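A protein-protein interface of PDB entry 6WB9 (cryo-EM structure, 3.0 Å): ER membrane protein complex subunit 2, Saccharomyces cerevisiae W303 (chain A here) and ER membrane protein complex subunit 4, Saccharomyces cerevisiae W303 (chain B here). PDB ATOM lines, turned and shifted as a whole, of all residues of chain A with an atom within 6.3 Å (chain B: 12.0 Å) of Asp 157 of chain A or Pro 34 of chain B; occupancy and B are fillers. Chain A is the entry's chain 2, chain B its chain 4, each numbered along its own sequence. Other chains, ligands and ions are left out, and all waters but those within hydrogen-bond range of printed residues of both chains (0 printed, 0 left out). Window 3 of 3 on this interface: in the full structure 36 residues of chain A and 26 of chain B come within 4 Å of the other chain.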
ATOM      1  N   LYS A 150      26.899   3.139 -15.195  1.00  0.00           N
ATOM      2  CA  LYS A 150      26.899   2.031 -14.243  1.00  0.00           C
ATOM      3  C   LYS A 150      27.070   2.529 -12.815  1.00  0.00           C
ATOM      4  O   LYS A 150      26.386   2.054 -11.901  1.00  0.00           O
ATOM      5  CB  LYS A 150      27.997   1.030 -14.607  1.00  0.00           C
ATOM      6  CG  LYS A 150      28.155  -0.113 -13.616  1.00  0.00           C
ATOM      7  CD  LYS A 150      28.730  -1.351 -14.282  1.00  0.00           C
ATOM      8  CE  LYS A 150      27.716  -1.985 -15.220  1.00  0.00           C
ATOM      9  NZ  LYS A 150      26.490  -2.419 -14.491  1.00  0.00           N
ATOM     10  N   VAL A 152      26.258   5.612 -11.727  1.00  0.00           N
ATOM     11  CA  VAL A 152      25.059   6.366 -11.357  1.00  0.00           C
ATOM     12  C   VAL A 152      23.879   5.423 -11.115  1.00  0.00           C
ATOM     13  O   VAL A 152      23.079   5.632 -10.193  1.00  0.00           O
ATOM     14  CB  VAL A 152      24.758   7.431 -12.432  1.00  0.00           C
ATOM     15  CG1 VAL A 152      23.413   8.099 -12.211  1.00  0.00           C
ATOM     16  CG2 VAL A 152      25.838   8.491 -12.420  1.00  0.00           C
ATOM     17  N   VAL A 153      23.785   4.338 -11.888  1.00  0.00           N
ATOM     18  CA  VAL A 153      22.732   3.349 -11.677  1.00  0.00           C
ATOM     19  C   VAL A 153      22.957   2.593 -10.368  1.00  0.00           C
ATOM     20  O   VAL A 153      21.999   2.295  -9.644  1.00  0.00           O
ATOM     21  CB  VAL A 153      22.648   2.427 -12.912  1.00  0.00           C
ATOM     22  CG1 VAL A 153      22.091   1.046 -12.584  1.00  0.00           C
ATOM     23  CG2 VAL A 153      21.789   3.082 -13.982  1.00  0.00           C
ATOM     24  N   ALA A 154      24.218   2.336 -10.004  1.00  0.00           N
ATOM     25  CA  ALA A 154      24.508   1.751  -8.700  1.00  0.00           C
ATOM     26  C   ALA A 154      24.215   2.723  -7.564  1.00  0.00           C
ATOM     27  O   ALA A 154      23.844   2.294  -6.467  1.00  0.00           O
ATOM     28  CB  ALA A 154      25.964   1.294  -8.640  1.00  0.00           C
ATOM     29  N   LEU A 155      24.373   4.027  -7.801  1.00  0.00           N
ATOM     30  CA  LEU A 155      24.011   5.021  -6.797  1.00  0.00           C
ATOM     31  C   LEU A 155      22.524   5.364  -6.807  1.00  0.00           C
ATOM     32  O   LEU A 155      22.075   6.144  -5.961  1.00  0.00           O
ATOM     33  CB  LEU A 155      24.846   6.291  -6.993  1.00  0.00           C
ATOM     34  CG  LEU A 155      25.129   7.126  -5.741  1.00  0.00           C
ATOM     35  CD1 LEU A 155      25.775   6.272  -4.673  1.00  0.00           C
ATOM     36  CD2 LEU A 155      25.976   8.329  -6.069  1.00  0.00           C
ATOM     37  N   THR A 156      21.752   4.836  -7.753  1.00  0.00           N
ATOM     38  CA  THR A 156      20.299   4.938  -7.669  1.00  0.00           C
ATOM     39  C   THR A 156      19.623   3.646  -7.225  1.00  0.00           C
ATOM     40  O   THR A 156      18.460   3.696  -6.810  1.00  0.00           O
ATOM     41  CB  THR A 156      19.689   5.364  -9.009  1.00  0.00           C
ATOM     42  OG1 THR A 156      20.112   4.466 -10.037  1.00  0.00           O
ATOM     43  CG2 THR A 156      20.098   6.769  -9.363  1.00  0.00           C
ATOM     44  N   ASP A 157      20.301   2.500  -7.338  1.00  0.00           N
ATOM     45  CA  ASP A 157      19.786   1.234  -6.822  1.00  0.00           C
ATOM     46  C   ASP A 157      19.657   1.314  -5.309  1.00  0.00           C
ATOM     47  O   ASP A 157      18.548   1.285  -4.772  1.00  0.00           O
ATOM     48  CB  ASP A 157      20.697   0.073  -7.223  1.00  0.00           C
ATOM     49  CG  ASP A 157      20.392  -0.459  -8.610  1.00  0.00           C
ATOM     50  OD1 ASP A 157      19.214  -0.763  -8.885  1.00  0.00           O
ATOM     51  OD2 ASP A 157      21.331  -0.571  -9.426  1.00  0.00           O
ATOM     52  N   LYS A 158      20.785   1.431  -4.617  1.00  0.00           N
ATOM     53  CA  LYS A 158      20.769   1.991  -3.279  1.00  0.00           C
ATOM     54  C   LYS A 158      20.635   3.497  -3.410  1.00  0.00           C
ATOM     55  O   LYS A 158      21.012   4.068  -4.430  1.00  0.00           O
ATOM     56  CB  LYS A 158      22.042   1.633  -2.510  1.00  0.00           C
ATOM     57  CG  LYS A 158      23.333   2.036  -3.200  1.00  0.00           C
ATOM     58  CD  LYS A 158      24.544   1.660  -2.366  1.00  0.00           C
ATOM     59  CE  LYS A 158      25.811   1.609  -3.204  1.00  0.00           C
ATOM     60  NZ  LYS A 158      26.136   2.921  -3.821  1.00  0.00           N
ATOM     61  N   PHE A 159      20.072   4.129  -2.377  1.00  0.00           N
ATOM     62  CA  PHE A 159      19.782   5.563  -2.311  1.00  0.00           C
ATOM     63  C   PHE A 159      18.989   6.112  -3.497  1.00  0.00           C
ATOM     64  O   PHE A 159      19.549   6.857  -4.312  1.00  0.00           O
ATOM     65  CB  PHE A 159      21.084   6.361  -2.182  1.00  0.00           C
ATOM     66  CG  PHE A 159      21.458   6.686  -0.773  1.00  0.00           C
ATOM     67  CD1 PHE A 159      21.387   5.725   0.219  1.00  0.00           C
ATOM     68  CD2 PHE A 159      21.898   7.951  -0.444  1.00  0.00           C
ATOM     69  CE1 PHE A 159      21.733   6.028   1.518  1.00  0.00           C
ATOM     70  CE2 PHE A 159      22.250   8.255   0.848  1.00  0.00           C
ATOM     71  CZ  PHE A 159      22.167   7.294   1.832  1.00  0.00           C
ATOM     72  N   PRO A 160      17.690   5.789  -3.641  1.00  0.00           N
ATOM     73  CA  PRO A 160      16.866   6.523  -4.610  1.00  0.00           C
ATOM     74  C   PRO A 160      16.394   7.846  -4.028  1.00  0.00           C
ATOM     75  O   PRO A 160      16.889   8.266  -2.977  1.00  0.00           O
ATOM     76  CB  PRO A 160      15.704   5.566  -4.875  1.00  0.00           C
ATOM     77  CG  PRO A 160      15.532   4.869  -3.592  1.00  0.00           C
ATOM     78  CD  PRO A 160      16.916   4.707  -3.006  1.00  0.00           C
ATOM     79  N   TRP A 166      19.111  10.907 -10.918  1.00  0.00           N
ATOM     80  CA  TRP A 166      18.232  10.554 -12.024  1.00  0.00           C
ATOM     81  C   TRP A 166      18.312  11.571 -13.155  1.00  0.00           C
ATOM     82  O   TRP A 166      18.189  11.198 -14.325  1.00  0.00           O
ATOM     83  CB  TRP A 166      16.796  10.424 -11.531  1.00  0.00           C
ATOM     84  CG  TRP A 166      16.573   9.296 -10.592  1.00  0.00           C
ATOM     85  CD1 TRP A 166      16.648   9.335  -9.233  1.00  0.00           C
ATOM     86  CD2 TRP A 166      16.228   7.954 -10.939  1.00  0.00           C
ATOM     87  NE1 TRP A 166      16.372   8.096  -8.711  1.00  0.00           N
ATOM     88  CE2 TRP A 166      16.113   7.230  -9.739  1.00  0.00           C
ATOM     89  CE3 TRP A 166      16.002   7.294 -12.150  1.00  0.00           C
ATOM     90  CZ2 TRP A 166      15.778   5.881  -9.714  1.00  0.00           C
ATOM     91  CZ3 TRP A 166      15.675   5.956 -12.123  1.00  0.00           C
ATOM     92  CH2 TRP A 166      15.563   5.264 -10.914  1.00  0.00           C
ATOM     93  N   TYR A 184      12.164   7.604 -18.528  1.00  0.00           N
ATOM     94  CA  TYR A 184      11.915   6.953 -17.245  1.00  0.00           C
ATOM     95  C   TYR A 184      12.605   7.691 -16.102  1.00  0.00           C
ATOM     96  O   TYR A 184      12.006   7.899 -15.036  1.00  0.00           O
ATOM     97  CB  TYR A 184      12.373   5.496 -17.298  1.00  0.00           C
ATOM     98  CG  TYR A 184      12.076   4.728 -16.033  1.00  0.00           C
ATOM     99  CD1 TYR A 184      10.790   4.293 -15.752  1.00  0.00           C
ATOM    100  CD2 TYR A 184      13.081   4.442 -15.119  1.00  0.00           C
ATOM    101  CE1 TYR A 184      10.510   3.596 -14.597  1.00  0.00           C
ATOM    102  CE2 TYR A 184      12.811   3.744 -13.960  1.00  0.00           C
ATOM    103  CZ  TYR A 184      11.524   3.323 -13.706  1.00  0.00           C
ATOM    104  OH  TYR A 184      11.244   2.629 -12.553  1.00  0.00           O
ATOM    105  N   THR B  29      25.606  -3.996 -22.897  1.00  0.00           N
ATOM    106  CA  THR B  29      25.946  -3.981 -21.483  1.00  0.00           C
ATOM    107  C   THR B  29      25.586  -2.656 -20.829  1.00  0.00           C
ATOM    108  O   THR B  29      26.055  -2.372 -19.722  1.00  0.00           O
ATOM    109  CB  THR B  29      27.435  -4.274 -21.288  1.00  0.00           C
ATOM    110  OG1 THR B  29      28.212  -3.307 -22.007  1.00  0.00           O
ATOM    111  CG2 THR B  29      27.773  -5.668 -21.793  1.00  0.00           C
ATOM    112  N   LEU B  30      24.781  -1.841 -21.498  1.00  0.00           N
ATOM    113  CA  LEU B  30      24.374  -0.546 -20.970  1.00  0.00           C
ATOM    114  C   LEU B  30      23.419  -0.742 -19.801  1.00  0.00           C
ATOM    115  O   LEU B  30      22.436  -1.481 -19.935  1.00  0.00           O
ATOM    116  CB  LEU B  30      23.711   0.282 -22.061  1.00  0.00           C
ATOM    117  CG  LEU B  30      23.551   1.767 -21.753  1.00  0.00           C
ATOM    118  CD1 LEU B  30      24.912   2.427 -21.686  1.00  0.00           C
ATOM    119  CD2 LEU B  30      22.693   2.427 -22.801  1.00  0.00           C
ATOM    120  N   PRO B  31      23.666  -0.120 -18.648  1.00  0.00           N
ATOM    121  CA  PRO B  31      22.810  -0.358 -17.478  1.00  0.00           C
ATOM    122  C   PRO B  31      21.476   0.364 -17.605  1.00  0.00           C
ATOM    123  O   PRO B  31      21.419   1.549 -17.937  1.00  0.00           O
ATOM    124  CB  PRO B  31      23.638   0.199 -16.315  1.00  0.00           C
ATOM    125  CG  PRO B  31      24.515   1.216 -16.944  1.00  0.00           C
ATOM    126  CD  PRO B  31      24.825   0.728 -18.324  1.00  0.00           C
ATOM    127  N   SER B  32      20.399  -0.370 -17.353  1.00  0.00           N
ATOM    128  CA  SER B  32      19.088   0.239 -17.260  1.00  0.00           C
ATOM    129  C   SER B  32      18.942   0.939 -15.908  1.00  0.00           C
ATOM    130  O   SER B  32      19.607   0.567 -14.938  1.00  0.00           O
ATOM    131  CB  SER B  32      18.003  -0.823 -17.422  1.00  0.00           C
ATOM    132  OG  SER B  32      18.077  -1.785 -16.386  1.00  0.00           O
ATOM    133  N   PRO B  33      18.096   1.963 -15.819  1.00  0.00           N
ATOM    134  CA  PRO B  33      17.767   2.535 -14.509  1.00  0.00           C
ATOM    135  C   PRO B  33      16.939   1.558 -13.693  1.00  0.00           C
ATOM    136  O   PRO B  33      16.371   0.608 -14.254  1.00  0.00           O
ATOM    137  CB  PRO B  33      16.962   3.796 -14.865  1.00  0.00           C
ATOM    138  CG  PRO B  33      16.440   3.540 -16.222  1.00  0.00           C
ATOM    139  CD  PRO B  33      17.490   2.739 -16.916  1.00  0.00           C
ATOM    140  N   PRO B  34      16.876   1.733 -12.357  1.00  0.00           N
ATOM    141  CA  PRO B  34      16.062   0.828 -11.532  1.00  0.00           C
ATOM    142  C   PRO B  34      14.577   0.879 -11.857  1.00  0.00           C
ATOM    143  O   PRO B  34      13.890   1.860 -11.559  1.00  0.00           O
ATOM    144  CB  PRO B  34      16.334   1.323 -10.107  1.00  0.00           C
ATOM    145  CG  PRO B  34      17.690   1.904 -10.179  1.00  0.00           C
ATOM    146  CD  PRO B  34      17.802   2.532 -11.536  1.00  0.00           C
ATOM    147  N   GLY B  35      14.085  -0.191 -12.461  1.00  0.00           N
ATOM    148  CA  GLY B  35      12.724  -0.274 -12.926  1.00  0.00           C
ATOM    149  C   GLY B  35      12.537  -0.258 -14.428  1.00  0.00           C
ATOM    150  O   GLY B  35      11.421   0.009 -14.888  1.00  0.00           O
ATOM    151  N   PHE B  36      13.580  -0.530 -15.202  1.00  0.00           N
ATOM    152  CA  PHE B  36      13.466  -0.527 -16.651  1.00  0.00           C
ATOM    153  C   PHE B  36      13.914  -1.867 -17.228  1.00  0.00           C
ATOM    154  O   PHE B  36      13.110  -2.617 -17.782  1.00  0.00           O
ATOM    155  CB  PHE B  36      14.288   0.615 -17.249  1.00  0.00           C
ATOM    156  CG  PHE B  36      13.909   0.961 -18.657  1.00  0.00           C
ATOM    157  CD1 PHE B  36      12.894   1.869 -18.906  1.00  0.00           C
ATOM    158  CD2 PHE B  36      14.567   0.383 -19.730  1.00  0.00           C
ATOM    159  CE1 PHE B  36      12.540   2.192 -20.202  1.00  0.00           C
ATOM    160  CE2 PHE B  36      14.218   0.701 -21.029  1.00  0.00           C
ATOM    161  CZ  PHE B  36      13.203   1.607 -21.264  1.00  0.00           C
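O of Val 152 of chain A lies within hydrogen-bond range of OG1 of Thr 156 of chain A.
O of Val 153 of chain A is in hydrogen-bond range of OG1 of Thr 156 of chain A (2.9 Å).
Asp 157 of chain A touches just one residue of chain B: Pro 34.
Printed residues of chain A within 4 Å of Pro 34 of chain B: Thr 156 (3.4 Å), Asp 157 (3.3 Å), Trp 166 (3.6 Å) and Tyr 184 (2.9 Å).
Val 153 of chain A touches just one residue of chain B: Ser 32.
No residue of chain B comes within 4 Å of Ala 154 of chain A.
Of chain B, only Pro 34 (3.4 Å) comes within 4 Å of Thr 156 of chain A.
No residue of chain B comes within 4 Å of Lys 158 of chain A.
No residue of chain B comes within 4 Å of Pro 160 of chain A.
Of the printed residues of chain A, Pro 31 of chain B touches Lys 150 (3.5 Å).
Printed residues of chain A within 4 Å of Ser 32 of chain B: Val 153.
Of the printed residues of chain B, Trp 166 of chain A touches Pro 33 (3.7 Å) and Pro 34 (3.6 Å).
Printed residues of chain B within 4 Å of Lys 150 of chain A: Pro 31.
Of the printed residues of chain A, Pro 33 of chain B touches Trp 166 (3.7 Å) and Tyr 184 (3.6 Å).
Phe 36 of chain B touches none of the printed residues of chain A.
Thr 29 of chain B touches none of the printed residues of chain A.
The nearest residue of chain B that does not touch Asp 157 of chain A is Pro 33 of chain B (5.8 Å).
The nearest residue of chain A that does not touch Pro 34 of chain B is Val 153 of chain A (4.4 Å).
The nearest printed residue of chain A that does not touch Pro 33 of chain B is Val 153 of chain A (4.1 Å).
O of Pro 34 of chain B lies within hydrogen-bond range of OH of Tyr 184 of chain A, at 2.9 Å.
Lys 150 of chain A touches Pro 31 of chain B.
Val 153 of chain A touches Ser 32 of chain B.
OG1 of Thr 156 of chain A touches CD of Pro 34 of chain B, at 3.4 Å.
CG of Pro 34 of chain B touches OD1 of Asp 157 of chain A (3.3 Å).
Trp 166 of chain A touches Pro 33 of chain B.
CH2 of Trp 166 of chain A touches CD of Pro 34 of chain B, at 3.6 Å.
CD2 of Tyr 184 of chain A touches CG of Pro 33 of chain B (3.6 Å).
Tyr 184 of chain A touches Gly 35 of chain B (OH to CA, 3.3 Å).
Hydrophobic or aromatic side chains of chain A that line the printed part of chain B: Val 153, Trp 166 and Tyr 184.
Hydrophobic or aromatic side chains of chain B that line the printed part of chain A: Pro 31, Pro 33 and Pro 34.
Along chain B the printed residues that touch a printed residue of chain A span positions 31 to 35.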
